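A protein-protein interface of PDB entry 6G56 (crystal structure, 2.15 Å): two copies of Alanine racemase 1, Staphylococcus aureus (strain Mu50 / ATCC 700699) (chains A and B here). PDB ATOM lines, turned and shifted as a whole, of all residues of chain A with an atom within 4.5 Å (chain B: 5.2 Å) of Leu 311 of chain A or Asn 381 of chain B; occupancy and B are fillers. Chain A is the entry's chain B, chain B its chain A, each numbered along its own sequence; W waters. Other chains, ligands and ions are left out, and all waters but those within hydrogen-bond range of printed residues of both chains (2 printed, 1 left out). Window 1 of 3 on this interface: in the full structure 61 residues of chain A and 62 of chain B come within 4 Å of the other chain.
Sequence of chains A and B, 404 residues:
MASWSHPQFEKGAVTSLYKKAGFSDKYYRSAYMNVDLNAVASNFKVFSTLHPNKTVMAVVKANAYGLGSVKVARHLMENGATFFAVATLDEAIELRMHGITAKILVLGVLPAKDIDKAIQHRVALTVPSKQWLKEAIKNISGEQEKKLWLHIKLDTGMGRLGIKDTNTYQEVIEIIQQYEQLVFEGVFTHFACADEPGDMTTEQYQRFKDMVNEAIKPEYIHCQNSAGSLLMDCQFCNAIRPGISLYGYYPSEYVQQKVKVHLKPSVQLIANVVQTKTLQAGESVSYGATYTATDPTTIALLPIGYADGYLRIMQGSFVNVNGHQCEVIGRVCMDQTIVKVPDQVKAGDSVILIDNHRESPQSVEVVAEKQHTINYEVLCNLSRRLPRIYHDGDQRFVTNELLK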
ATOM      1  N   TYR A 306      -5.346  11.475  31.150  1.00  0.00           N
ATOM      2  CA  TYR A 306      -4.322  12.258  30.450  1.00  0.00           C
ATOM      3  C   TYR A 306      -3.573  11.502  29.359  1.00  0.00           C
ATOM      4  O   TYR A 306      -3.085  12.140  28.421  1.00  0.00           O
ATOM      5  CB  TYR A 306      -3.354  13.003  31.423  1.00  0.00           C
ATOM      6  CG  TYR A 306      -2.489  12.181  32.329  1.00  0.00           C
ATOM      7  CD1 TYR A 306      -1.346  11.530  31.854  1.00  0.00           C
ATOM      8  CD2 TYR A 306      -2.757  12.103  33.690  1.00  0.00           C
ATOM      9  CE1 TYR A 306      -0.530  10.818  32.705  1.00  0.00           C
ATOM     10  CE2 TYR A 306      -1.952  11.371  34.553  1.00  0.00           C
ATOM     11  CZ  TYR A 306      -0.842  10.741  34.065  1.00  0.00           C
ATOM     12  OH  TYR A 306      -0.045  10.029  34.918  1.00  0.00           O
ATOM     13  N   GLY A 309      -5.181  12.485  26.261  1.00  0.00           N
ATOM     14  CA  GLY A 309      -5.074  13.911  25.978  1.00  0.00           C
ATOM     15  C   GLY A 309      -5.953  14.811  26.823  1.00  0.00           C
ATOM     16  O   GLY A 309      -6.021  16.025  26.565  1.00  0.00           O
ATOM     17  N   TYR A 310      -6.652  14.250  27.801  1.00  0.00           N
ATOM     18  CA  TYR A 310      -7.423  15.062  28.720  1.00  0.00           C
ATOM     19  C   TYR A 310      -6.494  15.311  29.894  1.00  0.00           C
ATOM     20  O   TYR A 310      -6.437  14.540  30.866  1.00  0.00           O
ATOM     21  CB  TYR A 310      -8.735  14.399  29.089  1.00  0.00           C
ATOM     22  CG  TYR A 310      -9.746  15.327  29.728  1.00  0.00           C
ATOM     23  CD1 TYR A 310     -10.456  16.254  28.961  1.00  0.00           C
ATOM     24  CD2 TYR A 310      -9.967  15.300  31.100  1.00  0.00           C
ATOM     25  CE1 TYR A 310     -11.368  17.115  29.546  1.00  0.00           C
ATOM     26  CE2 TYR A 310     -10.887  16.166  31.692  1.00  0.00           C
ATOM     27  CZ  TYR A 310     -11.589  17.056  30.912  1.00  0.00           C
ATOM     28  OH  TYR A 310     -12.483  17.903  31.503  1.00  0.00           O
ATOM     29  N   LEU A 311      -5.748  16.408  29.785  1.00  0.00           N
ATOM     30  CA  LEU A 311      -4.559  16.618  30.609  1.00  0.00           C
ATOM     31  C   LEU A 311      -4.850  16.930  32.071  1.00  0.00           C
ATOM     32  O   LEU A 311      -5.953  17.335  32.434  1.00  0.00           O
ATOM     33  CB  LEU A 311      -3.659  17.700  29.973  1.00  0.00           C
ATOM     34  CG  LEU A 311      -3.183  17.436  28.535  1.00  0.00           C
ATOM     35  CD1 LEU A 311      -2.196  18.501  28.082  1.00  0.00           C
ATOM     36  CD2 LEU A 311      -2.582  16.057  28.368  1.00  0.00           C
ATOM     37  N   ARG A 312      -3.836  16.742  32.902  1.00  0.00           N
ATOM     38  CA  ARG A 312      -3.943  16.949  34.345  1.00  0.00           C
ATOM     39  C   ARG A 312      -4.496  18.306  34.721  1.00  0.00           C
ATOM     40  O   ARG A 312      -5.285  18.433  35.659  1.00  0.00           O
ATOM     41  CB  ARG A 312      -2.591  16.726  35.006  1.00  0.00           C
ATOM     42  CG  ARG A 312      -2.266  15.237  35.021  1.00  0.00           C
ATOM     43  CD  ARG A 312      -0.882  14.961  35.546  1.00  0.00           C
ATOM     44  NE  ARG A 312      -0.802  15.009  37.001  1.00  0.00           N
ATOM     45  CZ  ARG A 312      -0.259  15.981  37.731  1.00  0.00           C
ATOM     46  NH1 ARG A 312       0.215  17.119  37.190  1.00  0.00           N
ATOM     47  NH2 ARG A 312      -0.204  15.814  39.052  1.00  0.00           N
ATOM     48  N   ILE A 313      -4.091  19.325  33.966  1.00  0.00           N
ATOM     49  CA  ILE A 313      -4.554  20.678  34.202  1.00  0.00           C
ATOM     50  C   ILE A 313      -6.092  20.815  34.091  1.00  0.00           C
ATOM     51  O   ILE A 313      -6.632  21.801  34.563  1.00  0.00           O
ATOM     52  CB  ILE A 313      -3.808  21.676  33.257  1.00  0.00           C
ATOM     53  CG1 ILE A 313      -3.926  23.116  33.734  1.00  0.00           C
ATOM     54  CG2 ILE A 313      -4.312  21.533  31.825  1.00  0.00           C
ATOM     55  CD1 ILE A 313      -3.006  24.083  32.987  1.00  0.00           C
ATOM     56  N   MET A 314      -6.806  19.842  33.503  1.00  0.00           N
ATOM     57  CA  MET A 314      -8.278  19.908  33.464  1.00  0.00           C
ATOM     58  C   MET A 314      -8.955  19.788  34.832  1.00  0.00           C
ATOM     59  O   MET A 314     -10.146  20.062  34.957  1.00  0.00           O
ATOM     60  CB  MET A 314      -8.856  18.863  32.514  1.00  0.00           C
ATOM     61  CG  MET A 314      -8.416  19.016  31.059  1.00  0.00           C
ATOM     62  SD  MET A 314      -8.646  20.680  30.384  1.00  0.00           S
ATOM     63  CE  MET A 314     -10.432  20.717  30.210  1.00  0.00           C
ATOM     64  N   VAL A 332      -6.552  14.367  37.816  1.00  0.00           N
ATOM     65  CA  VAL A 332      -6.896  13.644  36.623  1.00  0.00           C
ATOM     66  C   VAL A 332      -5.808  12.603  36.490  1.00  0.00           C
ATOM     67  O   VAL A 332      -4.634  12.901  36.579  1.00  0.00           O
ATOM     68  CB  VAL A 332      -6.924  14.547  35.382  1.00  0.00           C
ATOM     69  CG1 VAL A 332      -7.097  13.713  34.127  1.00  0.00           C
ATOM     70  CG2 VAL A 332      -8.031  15.575  35.509  1.00  0.00           C
ATOM     71  N   GLN A 371      -6.461  24.865  29.761  1.00  0.00           N
ATOM     72  CA  GLN A 371      -5.127  24.334  29.440  1.00  0.00           C
ATOM     73  C   GLN A 371      -4.018  25.395  29.263  1.00  0.00           C
ATOM     74  O   GLN A 371      -2.862  25.030  29.013  1.00  0.00           O
ATOM     75  CB  GLN A 371      -5.199  23.444  28.179  1.00  0.00           C
ATOM     76  CG  GLN A 371      -5.849  22.088  28.446  1.00  0.00           C
ATOM     77  CD  GLN A 371      -5.815  21.148  27.243  1.00  0.00           C
ATOM     78  OE1 GLN A 371      -4.992  21.292  26.338  1.00  0.00           O
ATOM     79  NE2 GLN A 371      -6.692  20.151  27.259  1.00  0.00           N
ATOM     80  N   ASN A 381      -3.768  17.213  21.116  1.00  0.00           N
ATOM     81  CA  ASN A 381      -3.474  16.383  22.306  1.00  0.00           C
ATOM     82  C   ASN A 381      -4.200  15.023  22.331  1.00  0.00           C
ATOM     83  O   ASN A 381      -3.755  14.080  23.012  1.00  0.00           O
ATOM     84  CB  ASN A 381      -3.904  17.114  23.578  1.00  0.00           C
ATOM     85  CG  ASN A 381      -2.922  18.191  24.040  1.00  0.00           C
ATOM     86  OD1 ASN A 381      -1.728  18.166  23.743  1.00  0.00           O
ATOM     87  ND2 ASN A 381      -3.440  19.119  24.834  1.00  0.00           N
ATOM     88  N   ASP B 308       3.338  16.740  17.871  1.00  0.00           N
ATOM     89  CA  ASP B 308       4.179  15.623  18.295  1.00  0.00           C
ATOM     90  C   ASP B 308       4.208  15.400  19.801  1.00  0.00           C
ATOM     91  O   ASP B 308       4.807  14.412  20.255  1.00  0.00           O
ATOM     92  CB  ASP B 308       5.579  15.807  17.760  1.00  0.00           C
ATOM     93  CG  ASP B 308       5.593  15.948  16.266  1.00  0.00           C
ATOM     94  OD1 ASP B 308       5.188  14.969  15.568  1.00  0.00           O
ATOM     95  OD2 ASP B 308       5.957  17.042  15.765  1.00  0.00           O
ATOM     96  N   GLY B 309       3.556  16.287  20.563  1.00  0.00           N
ATOM     97  CA  GLY B 309       3.596  16.273  22.022  1.00  0.00           C
ATOM     98  C   GLY B 309       4.662  17.157  22.657  1.00  0.00           C
ATOM     99  O   GLY B 309       4.860  17.119  23.879  1.00  0.00           O
ATOM    100  N   LEU B 311       4.906  20.371  23.615  1.00  0.00           N
ATOM    101  CA  LEU B 311       3.818  21.332  23.760  1.00  0.00           C
ATOM    102  C   LEU B 311       4.287  22.793  23.764  1.00  0.00           C
ATOM    103  O   LEU B 311       5.455  23.091  23.999  1.00  0.00           O
ATOM    104  CB  LEU B 311       3.009  21.033  25.027  1.00  0.00           C
ATOM    105  CG  LEU B 311       2.381  19.634  25.138  1.00  0.00           C
ATOM    106  CD1 LEU B 311       1.510  19.553  26.384  1.00  0.00           C
ATOM    107  CD2 LEU B 311       1.597  19.255  23.882  1.00  0.00           C
ATOM    108  N   GLN B 371       6.660  21.862  31.812  1.00  0.00           N
ATOM    109  CA  GLN B 371       5.255  21.608  31.480  1.00  0.00           C
ATOM    110  C   GLN B 371       4.257  21.772  32.625  1.00  0.00           C
ATOM    111  O   GLN B 371       3.038  21.602  32.412  1.00  0.00           O
ATOM    112  CB  GLN B 371       5.104  20.202  30.868  1.00  0.00           C
ATOM    113  CG  GLN B 371       5.619  20.104  29.443  1.00  0.00           C
ATOM    114  CD  GLN B 371       5.328  18.779  28.778  1.00  0.00           C
ATOM    115  OE1 GLN B 371       4.418  18.043  29.178  1.00  0.00           O
ATOM    116  NE2 GLN B 371       6.085  18.478  27.736  1.00  0.00           N
ATOM    117  N   GLU B 377       3.057  12.326  32.288  1.00  0.00           N
ATOM    118  CA  GLU B 377       2.316  13.019  31.234  1.00  0.00           C
ATOM    119  C   GLU B 377       3.203  13.438  30.077  1.00  0.00           C
ATOM    120  O   GLU B 377       2.738  13.443  28.926  1.00  0.00           O
ATOM    121  CB  GLU B 377       1.561  14.226  31.803  1.00  0.00           C
ATOM    122  CG  GLU B 377       0.544  14.841  30.848  1.00  0.00           C
ATOM    123  CD  GLU B 377      -0.225  15.981  31.467  1.00  0.00           C
ATOM    124  OE1 GLU B 377       0.369  17.022  31.750  1.00  0.00           O
ATOM    125  OE2 GLU B 377      -1.438  15.827  31.653  1.00  0.00           O
ATOM    126  N   VAL B 378       4.450  13.817  30.382  1.00  0.00           N
ATOM    127  CA  VAL B 378       5.448  14.150  29.350  1.00  0.00           C
ATOM    128  C   VAL B 378       5.527  12.990  28.362  1.00  0.00           C
ATOM    129  O   VAL B 378       5.442  13.190  27.155  1.00  0.00           O
ATOM    130  CB  VAL B 378       6.853  14.444  29.930  1.00  0.00           C
ATOM    131  CG1 VAL B 378       7.885  14.604  28.810  1.00  0.00           C
ATOM    132  CG2 VAL B 378       6.857  15.699  30.789  1.00  0.00           C
ATOM    133  N   LEU B 379       5.665  11.784  28.910  1.00  0.00           N
ATOM    134  CA  LEU B 379       5.752  10.573  28.134  1.00  0.00           C
ATOM    135  C   LEU B 379       4.477  10.280  27.357  1.00  0.00           C
ATOM    136  O   LEU B 379       4.545   9.995  26.164  1.00  0.00           O
ATOM    137  CB  LEU B 379       6.113   9.377  29.019  1.00  0.00           C
ATOM    138  CG  LEU B 379       7.490   9.402  29.694  1.00  0.00           C
ATOM    139  CD1 LEU B 379       7.605   8.284  30.725  1.00  0.00           C
ATOM    140  CD2 LEU B 379       8.606   9.304  28.656  1.00  0.00           C
ATOM    141  N   CYS B 380       3.328  10.397  28.015  1.00  0.00           N
ATOM    142  CA  CYS B 380       2.047  10.131  27.377  1.00  0.00           C
ATOM    143  C   CYS B 380       1.714  11.106  26.245  1.00  0.00           C
ATOM    144  O   CYS B 380       1.002  10.720  25.306  1.00  0.00           O
ATOM    145  CB  CYS B 380       0.909  10.103  28.408  1.00  0.00           C
ATOM    146  SG  CYS B 380       0.998   8.642  29.481  1.00  0.00           S
ATOM    147  N   ASN B 381       2.196  12.345  26.347  1.00  0.00           N
ATOM    148  CA  ASN B 381       1.945  13.382  25.321  1.00  0.00           C
ATOM    149  C   ASN B 381       2.512  13.054  23.922  1.00  0.00           C
ATOM    150  O   ASN B 381       2.022  13.580  22.900  1.00  0.00           O
ATOM    151  CB  ASN B 381       2.568  14.716  25.735  1.00  0.00           C
ATOM    152  CG  ASN B 381       1.776  15.475  26.782  1.00  0.00           C
ATOM    153  OD1 ASN B 381       0.554  15.336  26.908  1.00  0.00           O
ATOM    154  ND2 ASN B 381       2.485  16.363  27.515  1.00  0.00           N
ATOM    155  N   LEU B 382       3.571  12.251  23.892  1.00  0.00           N
ATOM    156  CA  LEU B 382       4.323  12.011  22.698  1.00  0.00           C
ATOM    157  C   LEU B 382       3.451  11.242  21.692  1.00  0.00           C
ATOM    158  O   LEU B 382       3.018  10.104  21.929  1.00  0.00           O
ATOM    159  CB  LEU B 382       5.620  11.286  23.010  1.00  0.00           C
ATOM    160  CG  LEU B 382       6.548  12.035  23.965  1.00  0.00           C
ATOM    161  CD1 LEU B 382       7.778  11.229  24.344  1.00  0.00           C
ATOM    162  CD2 LEU B 382       6.948  13.406  23.396  1.00  0.00           C
ATOM    163  N   SER B 383       3.180  11.908  20.577  1.00  0.00           N
ATOM    164  CA  SER B 383       2.099  11.499  19.701  1.00  0.00           C
ATOM    165  C   SER B 383       2.524  10.392  18.744  1.00  0.00           C
ATOM    166  O   SER B 383       3.710  10.085  18.604  1.00  0.00           O
ATOM    167  CB  SER B 383       1.580  12.716  18.909  1.00  0.00           C
ATOM    168  OG  SER B 383       2.313  12.887  17.731  1.00  0.00           O
HETATM  169  O   HOH W   1      -1.321  19.070  32.573  1.00  0.00           O
HETATM  170  O   HOH W   2      -0.837  15.548  24.522  1.00  0.00           O
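Leu 311 of chain A touches Asn 381 of chain B, and with the chains exchanged Asn 381 of chain A touches Leu 311 of chain B.
Of the 5 pairs that touch across the chains among the printed residues, 2 have their exchanged pair printed and touching as well.
The side-chain amide nitrogen (ND2) of Asn 381 of chain B sits close to the backbone carbonyl oxygen (O) of Glu 377 of chain B (3.3 Å).
ND2 of Asn 381 of chain A is in hydrogen-bond range of OE1 of Gln 371 of chain A, at 3.1 Å.
The side-chain amide oxygen of Gln 371 of chain B is in hydrogen-bond range of the side-chain amide nitrogen of Asn 381 of chain B (3.1 Å).
Water W2 bridges OD1 of Asn 381 of chain B (2.8 Å) and OD1 of Asn 381 of chain A (2.9 Å).
Water W1 lies within hydrogen-bond range of OE1 of Glu 377 of chain B, N of Ile 313 of chain A and N of Arg 312 of chain A.
The side-chain carboxylate of Glu 377 of chain B sits at hydrogen-bond distance from the backbone NH of Arg 312 of chain A.
Printed residues of chain B that touch a printed residue of chain A: Leu 311, Glu 377 and Asn 381.
Hydrophobic or aromatic side chains of chain B within 4 Å of the printed part of chain A: Leu 311.
Of the 10 printed residues of chain A, 4 touch a printed residue of chain B.
Printed residues of chain A that touch a printed residue of chain B: Tyr 306, Leu 311, Arg 312 and Asn 381.
Hydrophobic or aromatic side chains of chain A within 4 Å of the printed part of chain B: Tyr 306 and Leu 311.
Among the printed residues, merely in contact across the chains: Tyr 306 of chain A with Glu 377 of chain B (3.4 Å), Leu 311 of chain A with Glu 377 of chain B (3.4 Å), Leu 311 of chain A with Asn 381 of chain B (3.5 Å) and Asn 381 of chain A with Leu 311 of chain B (3.5 Å).
Of the printed residues of chain B, Tyr 306 of chain A touches Glu 377 (3.4 Å).
Of chain B, only Glu 377 (3.4 Å) and Asn 381 (3.5 Å) come within 4 Å of Leu 311 of chain A.
Printed residues of chain B within 4 Å of Arg 312 of chain A: Glu 377.
Of the printed residues of chain B, Asn 381 of chain A touches Leu 311 (3.5 Å).
Printed residues of chain A within 4 Å of Leu 311 of chain B: Asn 381 (3.5 Å).
Of the printed residues of chain A, Glu 377 of chain B touches Tyr 306 (3.4 Å), Leu 311 (3.4 Å) and Arg 312 (2.9 Å).
Asn 381 of chain B touches one residue of chain A.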
